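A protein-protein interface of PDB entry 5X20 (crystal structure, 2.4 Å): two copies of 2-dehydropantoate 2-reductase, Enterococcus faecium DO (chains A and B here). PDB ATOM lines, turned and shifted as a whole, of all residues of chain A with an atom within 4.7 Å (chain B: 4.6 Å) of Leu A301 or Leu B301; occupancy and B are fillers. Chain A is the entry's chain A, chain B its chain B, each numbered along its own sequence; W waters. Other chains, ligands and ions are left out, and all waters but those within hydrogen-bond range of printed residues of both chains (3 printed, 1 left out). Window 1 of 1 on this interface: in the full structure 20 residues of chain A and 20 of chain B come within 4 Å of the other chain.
O of Leu A201 lies within hydrogen-bond range of NZ of Lys B305 (3.1 Å). The side-chain amino group (NZ) of Lys A305 is in hydrogen-bond range of the backbone carbonyl oxygen (O) of Leu B201 (3.1 Å).
Of the printed residues of chain B, Leu A197 touches Phe B297. Thr A299 touches none of the printed residues of chain B. Of the printed residues of chain B, Leu A301 touches Leu B197, Leu B201, Met B217 and Leu B301. Printed residues of chain A within 4 Å of Met B217: Phe A297, Glu A300, Leu A301 and Ala A304. Of the printed residues of chain A, Phe B297 touches Leu A197, Met A217, Phe A297 and Leu A298. Printed residues of chain A within 4 Å of Leu B301: Leu A201, Met A217 and Leu A301. Of the printed residues of chain A, Ala B304 touches Leu A201. Printed residues of chain A within 4 Å of Lys B305: Leu A201 (3.1 Å). The nearest residue of chain A that does not touch Leu B301 is Leu A197 (4.02 Å).
Leu A197 touches Phe B297, but with the chains exchanged Phe A297 does not touch Leu B197 (4.02 Å). Ile B200 touches its own counterpart, Ile A200. Ile A200 touches Leu B201, and with the chains exchanged Leu A201 touches Ile B200. Phe B297 touches its own counterpart, Phe A297. Positions printed for both chains: 197, 200, 201, 217, 297, 298, 299, 300, 301, 302, 303, 304 and 305. Of the 22 pairs that touch across the chains among the printed residues, 19 have their exchanged pair printed and touching as well.
Of the 13 printed residues of chain B, 10 touch a printed residue of chain A. Hydrophobic or aromatic side chains of chain B that line the printed part of chain A: Leu B197, Ile B200, Leu B201, Met B217, Phe B297, Leu B298, Leu B301 and Ala B304. Along chain B the printed residues that touch a printed residue of chain A span positions 197 to 305. Of the 13 printed residues of chain A, 10 touch a printed residue of chain B. Hydrophobic or aromatic side chains of chain A within 4 Å of the printed part of chain B: Leu A197, Ile A200, Leu A201, Met A217, Phe A297, Leu A298, Leu A301 and Ala A304. Among the printed residues, no Asp or Glu carboxylate lies within 4 Å of a Lys or Arg side-chain nitrogen of the other chain.
CG2 of Ile B200 touches CG2 of Ile A200 (3.4 Å). Leu A201 touches Ala B304. Glu B300 touches Met A217. Met A217 touches Leu B301. Phe A297 touches Met B217 (CE1 to SD, 3.7 Å). CD2 of Phe A297 touches CD2 of Phe B297 (3.8 Å). Met B217 touches Glu A300 (CG to OE1, 3.7 Å). Leu A301 touches Met B217 (CD2 to SD, 3.7 Å). CB of Ala A304 touches CD1 of Leu B201, at 3.9 Å. Ala A304 touches Met B217 (CB to CE, 3.99 Å).
Water W1 lies within hydrogen-bond range of the side-chain amino group (NZ) of Lys B305, the backbone carbonyl oxygen (O) of Ile A200 and the backbone carbonyl oxygen (O) of Leu A201. Water W3 lies within hydrogen-bond range of O of Leu B201 (2.9 Å) and NZ of Lys A305 (2.9 Å). Water W2 lies within hydrogen-bond range of NZ of Lys B305 (3.0 Å) and O of Leu A201 (3.0 Å).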
ATOM      1  N   LEU A 197      19.487 -13.304   1.453  1.00  0.00           N
ATOM      2  CA  LEU A 197      19.252 -13.738   0.071  1.00  0.00           C
ATOM      3  C   LEU A 197      20.135 -14.937  -0.339  1.00  0.00           C
ATOM      4  O   LEU A 197      19.628 -15.909  -0.914  1.00  0.00           O
ATOM      5  CB  LEU A 197      19.410 -12.600  -0.914  1.00  0.00           C
ATOM      6  CG  LEU A 197      18.449 -11.446  -0.786  1.00  0.00           C
ATOM      7  CD1 LEU A 197      18.862 -10.353  -1.773  1.00  0.00           C
ATOM      8  CD2 LEU A 197      17.020 -11.885  -1.036  1.00  0.00           C
ATOM      9  N   ILE A 200      18.788 -18.110   1.573  1.00  0.00           N
ATOM     10  CA  ILE A 200      17.510 -18.612   1.083  1.00  0.00           C
ATOM     11  C   ILE A 200      17.661 -19.162  -0.313  1.00  0.00           C
ATOM     12  O   ILE A 200      17.054 -20.200  -0.651  1.00  0.00           O
ATOM     13  CB  ILE A 200      16.414 -17.511   1.172  1.00  0.00           C
ATOM     14  CG1 ILE A 200      15.916 -17.391   2.608  1.00  0.00           C
ATOM     15  CG2 ILE A 200      15.241 -17.796   0.277  1.00  0.00           C
ATOM     16  CD1 ILE A 200      15.250 -18.630   3.151  1.00  0.00           C
ATOM     17  N   LEU A 201      18.493 -18.526  -1.126  1.00  0.00           N
ATOM     18  CA  LEU A 201      18.623 -18.965  -2.511  1.00  0.00           C
ATOM     19  C   LEU A 201      19.664 -20.032  -2.726  1.00  0.00           C
ATOM     20  O   LEU A 201      19.734 -20.613  -3.807  1.00  0.00           O
ATOM     21  CB  LEU A 201      18.884 -17.783  -3.416  1.00  0.00           C
ATOM     22  CG  LEU A 201      17.661 -16.901  -3.575  1.00  0.00           C
ATOM     23  CD1 LEU A 201      18.097 -15.590  -4.195  1.00  0.00           C
ATOM     24  CD2 LEU A 201      16.597 -17.579  -4.433  1.00  0.00           C
ATOM     25  N   MET A 217      15.604  -6.743  -5.736  1.00  0.00           N
ATOM     26  CA  MET A 217      15.493  -7.169  -4.348  1.00  0.00           C
ATOM     27  C   MET A 217      16.387  -6.322  -3.454  1.00  0.00           C
ATOM     28  O   MET A 217      15.964  -5.860  -2.394  1.00  0.00           O
ATOM     29  CB  MET A 217      15.810  -8.671  -4.210  1.00  0.00           C
ATOM     30  CG  MET A 217      14.801  -9.559  -4.984  1.00  0.00           C
ATOM     31  SD  MET A 217      14.972 -11.341  -4.646  1.00  0.00           S
ATOM     32  CE  MET A 217      16.505 -11.665  -5.531  1.00  0.00           C
ATOM     33  N   PHE A 297       9.327 -10.412   5.295  1.00  0.00           N
ATOM     34  CA  PHE A 297       9.210 -11.682   4.575  1.00  0.00           C
ATOM     35  C   PHE A 297      10.549 -12.441   4.608  1.00  0.00           C
ATOM     36  O   PHE A 297      10.592 -13.649   4.854  1.00  0.00           O
ATOM     37  CB  PHE A 297       8.769 -11.402   3.129  1.00  0.00           C
ATOM     38  CG  PHE A 297       8.264 -12.611   2.344  1.00  0.00           C
ATOM     39  CD1 PHE A 297       8.021 -13.830   2.929  1.00  0.00           C
ATOM     40  CD2 PHE A 297       7.916 -12.459   1.023  1.00  0.00           C
ATOM     41  CE1 PHE A 297       7.561 -14.890   2.194  1.00  0.00           C
ATOM     42  CE2 PHE A 297       7.398 -13.505   0.274  1.00  0.00           C
ATOM     43  CZ  PHE A 297       7.237 -14.714   0.844  1.00  0.00           C
ATOM     44  N   LEU A 298      11.656 -11.720   4.401  1.00  0.00           N
ATOM     45  CA  LEU A 298      12.973 -12.368   4.440  1.00  0.00           C
ATOM     46  C   LEU A 298      13.298 -12.959   5.807  1.00  0.00           C
ATOM     47  O   LEU A 298      13.786 -14.081   5.929  1.00  0.00           O
ATOM     48  CB  LEU A 298      14.064 -11.437   3.959  1.00  0.00           C
ATOM     49  CG  LEU A 298      15.454 -12.045   3.849  1.00  0.00           C
ATOM     50  CD1 LEU A 298      15.549 -13.219   2.895  1.00  0.00           C
ATOM     51  CD2 LEU A 298      16.418 -10.994   3.423  1.00  0.00           C
ATOM     52  N   THR A 299      12.938 -12.238   6.852  1.00  0.00           N
ATOM     53  CA  THR A 299      13.060 -12.742   8.199  1.00  0.00           C
ATOM     54  C   THR A 299      12.233 -13.992   8.471  1.00  0.00           C
ATOM     55  O   THR A 299      12.712 -14.970   9.023  1.00  0.00           O
ATOM     56  CB  THR A 299      12.658 -11.662   9.201  1.00  0.00           C
ATOM     57  OG1 THR A 299      13.494 -10.501   9.023  1.00  0.00           O
ATOM     58  CG2 THR A 299      12.861 -12.143  10.621  1.00  0.00           C
ATOM     59  N   GLU A 300      10.988 -13.953   8.048  1.00  0.00           N
ATOM     60  CA  GLU A 300      10.102 -15.093   8.124  1.00  0.00           C
ATOM     61  C   GLU A 300      10.636 -16.328   7.358  1.00  0.00           C
ATOM     62  O   GLU A 300      10.572 -17.463   7.860  1.00  0.00           O
ATOM     63  CB  GLU A 300       8.734 -14.741   7.584  1.00  0.00           C
ATOM     64  CG  GLU A 300       7.964 -13.876   8.558  1.00  0.00           C
ATOM     65  CD  GLU A 300       6.838 -13.052   7.935  1.00  0.00           C
ATOM     66  OE1 GLU A 300       6.632 -13.002   6.701  1.00  0.00           O
ATOM     67  OE2 GLU A 300       6.110 -12.379   8.686  1.00  0.00           O
ATOM     68  N   LEU A 301      11.100 -16.083   6.140  1.00  0.00           N
ATOM     69  CA  LEU A 301      11.687 -17.146   5.319  1.00  0.00           C
ATOM     70  C   LEU A 301      12.907 -17.763   5.984  1.00  0.00           C
ATOM     71  O   LEU A 301      13.069 -18.963   5.969  1.00  0.00           O
ATOM     72  CB  LEU A 301      12.079 -16.617   3.914  1.00  0.00           C
ATOM     73  CG  LEU A 301      10.860 -16.358   3.045  1.00  0.00           C
ATOM     74  CD1 LEU A 301      11.244 -15.509   1.843  1.00  0.00           C
ATOM     75  CD2 LEU A 301      10.193 -17.658   2.579  1.00  0.00           C
ATOM     76  N   VAL A 302      13.783 -16.939   6.530  1.00  0.00           N
ATOM     77  CA  VAL A 302      14.984 -17.468   7.159  1.00  0.00           C
ATOM     78  C   VAL A 302      14.625 -18.297   8.390  1.00  0.00           C
ATOM     79  O   VAL A 302      15.187 -19.365   8.603  1.00  0.00           O
ATOM     80  CB  VAL A 302      15.970 -16.346   7.482  1.00  0.00           C
ATOM     81  CG1 VAL A 302      17.136 -16.836   8.350  1.00  0.00           C
ATOM     82  CG2 VAL A 302      16.528 -15.804   6.190  1.00  0.00           C
ATOM     83  N   HIS A 303      13.696 -17.810   9.214  1.00  0.00           N
ATOM     84  CA  HIS A 303      13.231 -18.609  10.384  1.00  0.00           C
ATOM     85  C   HIS A 303      12.631 -19.922   9.911  1.00  0.00           C
ATOM     86  O   HIS A 303      12.820 -20.974  10.556  1.00  0.00           O
ATOM     87  CB  HIS A 303      12.227 -17.842  11.292  1.00  0.00           C
ATOM     88  CG  HIS A 303      12.865 -16.763  12.098  1.00  0.00           C
ATOM     89  ND1 HIS A 303      14.062 -16.945  12.752  1.00  0.00           N
ATOM     90  CD2 HIS A 303      12.495 -15.482  12.348  1.00  0.00           C
ATOM     91  CE1 HIS A 303      14.424 -15.812  13.345  1.00  0.00           C
ATOM     92  NE2 HIS A 303      13.480 -14.915  13.118  1.00  0.00           N
ATOM     93  N   ALA A 304      11.875 -19.870   8.818  1.00  0.00           N
ATOM     94  CA  ALA A 304      11.254 -21.092   8.328  1.00  0.00           C
ATOM     95  C   ALA A 304      12.356 -22.061   7.882  1.00  0.00           C
ATOM     96  O   ALA A 304      12.251 -23.246   8.060  1.00  0.00           O
ATOM     97  CB  ALA A 304      10.281 -20.840   7.208  1.00  0.00           C
ATOM     98  N   LYS A 305      13.367 -21.527   7.256  1.00  0.00           N
ATOM     99  CA  LYS A 305      14.444 -22.333   6.816  1.00  0.00           C
ATOM    100  C   LYS A 305      15.159 -22.997   7.982  1.00  0.00           C
ATOM    101  O   LYS A 305      15.410 -24.216   7.947  1.00  0.00           O
ATOM    102  CB  LYS A 305      15.417 -21.498   5.998  1.00  0.00           C
ATOM    103  CG  LYS A 305      16.513 -22.334   5.352  1.00  0.00           C
ATOM    104  CD  LYS A 305      15.912 -23.231   4.282  1.00  0.00           C
ATOM    105  CE  LYS A 305      16.985 -24.141   3.734  1.00  0.00           C
ATOM    106  NZ  LYS A 305      16.474 -24.909   2.581  1.00  0.00           N
ATOM    107  N   LEU B 197       6.558 -21.067  -1.827  1.00  0.00           N
ATOM    108  CA  LEU B 197       7.195 -21.254  -0.527  1.00  0.00           C
ATOM    109  C   LEU B 197       7.895 -22.617  -0.424  1.00  0.00           C
ATOM    110  O   LEU B 197       9.050 -22.667   0.020  1.00  0.00           O
ATOM    111  CB  LEU B 197       6.197 -21.099   0.605  1.00  0.00           C
ATOM    112  CG  LEU B 197       5.566 -19.728   0.790  1.00  0.00           C
ATOM    113  CD1 LEU B 197       4.558 -19.780   1.904  1.00  0.00           C
ATOM    114  CD2 LEU B 197       6.626 -18.678   1.101  1.00  0.00           C
ATOM    115  N   ILE B 200      11.070 -22.400  -2.745  1.00  0.00           N
ATOM    116  CA  ILE B 200      12.180 -21.583  -2.195  1.00  0.00           C
ATOM    117  C   ILE B 200      12.765 -22.185  -0.936  1.00  0.00           C
ATOM    118  O   ILE B 200      13.936 -22.155  -0.704  1.00  0.00           O
ATOM    119  CB  ILE B 200      11.665 -20.133  -1.957  1.00  0.00           C
ATOM    120  CG1 ILE B 200      11.635 -19.358  -3.294  1.00  0.00           C
ATOM    121  CG2 ILE B 200      12.555 -19.364  -1.024  1.00  0.00           C
ATOM    122  CD1 ILE B 200      12.981 -19.195  -3.982  1.00  0.00           C
ATOM    123  N   LEU B 201      11.933 -22.789  -0.109  1.00  0.00           N
ATOM    124  CA  LEU B 201      12.377 -23.311   1.206  1.00  0.00           C
ATOM    125  C   LEU B 201      12.835 -24.747   1.132  1.00  0.00           C
ATOM    126  O   LEU B 201      13.475 -25.233   2.063  1.00  0.00           O
ATOM    127  CB  LEU B 201      11.284 -23.157   2.247  1.00  0.00           C
ATOM    128  CG  LEU B 201      11.086 -21.748   2.662  1.00  0.00           C
ATOM    129  CD1 LEU B 201       9.792 -21.676   3.440  1.00  0.00           C
ATOM    130  CD2 LEU B 201      12.257 -21.212   3.489  1.00  0.00           C
ATOM    131  N   MET B 217       3.182 -16.106   6.755  1.00  0.00           N
ATOM    132  CA  MET B 217       3.497 -15.910   5.362  1.00  0.00           C
ATOM    133  C   MET B 217       2.253 -16.193   4.551  1.00  0.00           C
ATOM    134  O   MET B 217       1.911 -15.418   3.647  1.00  0.00           O
ATOM    135  CB  MET B 217       4.671 -16.807   4.923  1.00  0.00           C
ATOM    136  CG  MET B 217       5.971 -16.426   5.593  1.00  0.00           C
ATOM    137  SD  MET B 217       7.421 -17.308   4.986  1.00  0.00           S
ATOM    138  CE  MET B 217       7.165 -18.935   5.611  1.00  0.00           C
ATOM    139  N   PHE B 297       8.072 -10.102  -4.034  1.00  0.00           N
ATOM    140  CA  PHE B 297       9.314 -10.656  -3.537  1.00  0.00           C
ATOM    141  C   PHE B 297       9.362 -12.177  -3.865  1.00  0.00           C
ATOM    142  O   PHE B 297      10.402 -12.706  -4.307  1.00  0.00           O
ATOM    143  CB  PHE B 297       9.408 -10.411  -2.009  1.00  0.00           C
ATOM    144  CG  PHE B 297      10.782 -10.619  -1.408  1.00  0.00           C
ATOM    145  CD1 PHE B 297      11.933 -10.818  -2.201  1.00  0.00           C
ATOM    146  CD2 PHE B 297      10.951 -10.480  -0.067  1.00  0.00           C
ATOM    147  CE1 PHE B 297      13.182 -10.934  -1.634  1.00  0.00           C
ATOM    148  CE2 PHE B 297      12.200 -10.619   0.517  1.00  0.00           C
ATOM    149  CZ  PHE B 297      13.308 -10.886  -0.270  1.00  0.00           C
ATOM    150  N   LEU B 298       8.252 -12.875  -3.662  1.00  0.00           N
ATOM    151  CA  LEU B 298       8.241 -14.334  -3.925  1.00  0.00           C
ATOM    152  C   LEU B 298       8.467 -14.622  -5.393  1.00  0.00           C
ATOM    153  O   LEU B 298       9.238 -15.545  -5.765  1.00  0.00           O
ATOM    154  CB  LEU B 298       6.998 -14.998  -3.400  1.00  0.00           C
ATOM    155  CG  LEU B 298       6.952 -16.508  -3.542  1.00  0.00           C
ATOM    156  CD1 LEU B 298       8.046 -17.227  -2.793  1.00  0.00           C
ATOM    157  CD2 LEU B 298       5.609 -17.014  -3.017  1.00  0.00           C
ATOM    158  N   THR B 299       7.879 -13.805  -6.237  1.00  0.00           N
ATOM    159  CA  THR B 299       8.094 -13.945  -7.670  1.00  0.00           C
ATOM    160  C   THR B 299       9.563 -13.683  -8.069  1.00  0.00           C
ATOM    161  O   THR B 299      10.168 -14.449  -8.838  1.00  0.00           O
ATOM    162  CB  THR B 299       7.192 -12.980  -8.437  1.00  0.00           C
ATOM    163  OG1 THR B 299       5.829 -13.265  -8.125  1.00  0.00           O
ATOM    164  CG2 THR B 299       7.382 -13.118  -9.933  1.00  0.00           C
ATOM    165  N   GLU B 300      10.123 -12.633  -7.517  1.00  0.00           N
ATOM    166  CA  GLU B 300      11.543 -12.342  -7.702  1.00  0.00           C
ATOM    167  C   GLU B 300      12.454 -13.451  -7.232  1.00  0.00           C
ATOM    168  O   GLU B 300      13.466 -13.771  -7.897  1.00  0.00           O
ATOM    169  CB  GLU B 300      11.893 -11.053  -6.977  1.00  0.00           C
ATOM    170  CG  GLU B 300      11.331  -9.841  -7.723  1.00  0.00           C
ATOM    171  CD  GLU B 300      10.996  -8.648  -6.854  1.00  0.00           C
ATOM    172  OE1 GLU B 300      11.327  -8.577  -5.633  1.00  0.00           O
ATOM    173  OE2 GLU B 300      10.389  -7.712  -7.423  1.00  0.00           O
ATOM    174  N   LEU B 301      12.139 -13.988  -6.053  1.00  0.00           N
ATOM    175  CA  LEU B 301      12.945 -15.067  -5.472  1.00  0.00           C
ATOM    176  C   LEU B 301      12.896 -16.306  -6.329  1.00  0.00           C
ATOM    177  O   LEU B 301      13.927 -16.929  -6.563  1.00  0.00           O
ATOM    178  CB  LEU B 301      12.484 -15.394  -4.055  1.00  0.00           C
ATOM    179  CG  LEU B 301      12.899 -14.366  -3.043  1.00  0.00           C
ATOM    180  CD1 LEU B 301      12.121 -14.585  -1.765  1.00  0.00           C
ATOM    181  CD2 LEU B 301      14.386 -14.398  -2.746  1.00  0.00           C
ATOM    182  N   VAL B 302      11.721 -16.652  -6.841  1.00  0.00           N
ATOM    183  CA  VAL B 302      11.618 -17.815  -7.694  1.00  0.00           C
ATOM    184  C   VAL B 302      12.431 -17.588  -8.987  1.00  0.00           C
ATOM    185  O   VAL B 302      13.074 -18.534  -9.455  1.00  0.00           O
ATOM    186  CB  VAL B 302      10.155 -18.186  -7.925  1.00  0.00           C
ATOM    187  CG1 VAL B 302       9.971 -19.260  -8.967  1.00  0.00           C
ATOM    188  CG2 VAL B 302       9.565 -18.669  -6.631  1.00  0.00           C
ATOM    189  N   HIS B 303      12.353 -16.402  -9.598  1.00  0.00           N
ATOM    190  CA  HIS B 303      13.071 -16.141 -10.868  1.00  0.00           C
ATOM    191  C   HIS B 303      14.543 -16.178 -10.603  1.00  0.00           C
ATOM    192  O   HIS B 303      15.313 -16.749 -11.414  1.00  0.00           O
ATOM    193  CB  HIS B 303      12.703 -14.816 -11.542  1.00  0.00           C
ATOM    194  CG  HIS B 303      11.347 -14.830 -12.190  1.00  0.00           C
ATOM    195  ND1 HIS B 303      10.905 -15.877 -12.970  1.00  0.00           N
ATOM    196  CD2 HIS B 303      10.344 -13.916 -12.187  1.00  0.00           C
ATOM    197  CE1 HIS B 303       9.689 -15.612 -13.419  1.00  0.00           C
ATOM    198  NE2 HIS B 303       9.320 -14.431 -12.936  1.00  0.00           N
ATOM    199  N   ALA B 304      14.938 -15.721  -9.424  1.00  0.00           N
ATOM    200  CA  ALA B 304      16.368 -15.755  -9.082  1.00  0.00           C
ATOM    201  C   ALA B 304      16.801 -17.202  -8.900  1.00  0.00           C
ATOM    202  O   ALA B 304      17.876 -17.589  -9.306  1.00  0.00           O
ATOM    203  CB  ALA B 304      16.677 -14.962  -7.827  1.00  0.00           C
ATOM    204  N   LYS B 305      15.951 -18.003  -8.290  1.00  0.00           N
ATOM    205  CA  LYS B 305      16.248 -19.404  -8.136  1.00  0.00           C
ATOM    206  C   LYS B 305      16.404 -20.079  -9.468  1.00  0.00           C
ATOM    207  O   LYS B 305      17.361 -20.862  -9.685  1.00  0.00           O
ATOM    208  CB  LYS B 305      15.170 -20.075  -7.308  1.00  0.00           C
ATOM    209  CG  LYS B 305      15.479 -21.502  -6.942  1.00  0.00           C
ATOM    210  CD  LYS B 305      16.649 -21.554  -5.999  1.00  0.00           C
ATOM    211  CE  LYS B 305      17.044 -23.001  -5.741  1.00  0.00           C
ATOM    212  NZ  LYS B 305      18.086 -23.054  -4.677  1.00  0.00           N
HETATM  213  O   HOH W   1      16.906 -22.088  -2.569  1.00  0.00           O
HETATM  214  O   HOH W   2      20.527 -22.318  -6.186  1.00  0.00           O
HETATM  215  O   HOH W   3      14.888 -26.977   3.875  1.00  0.00           O
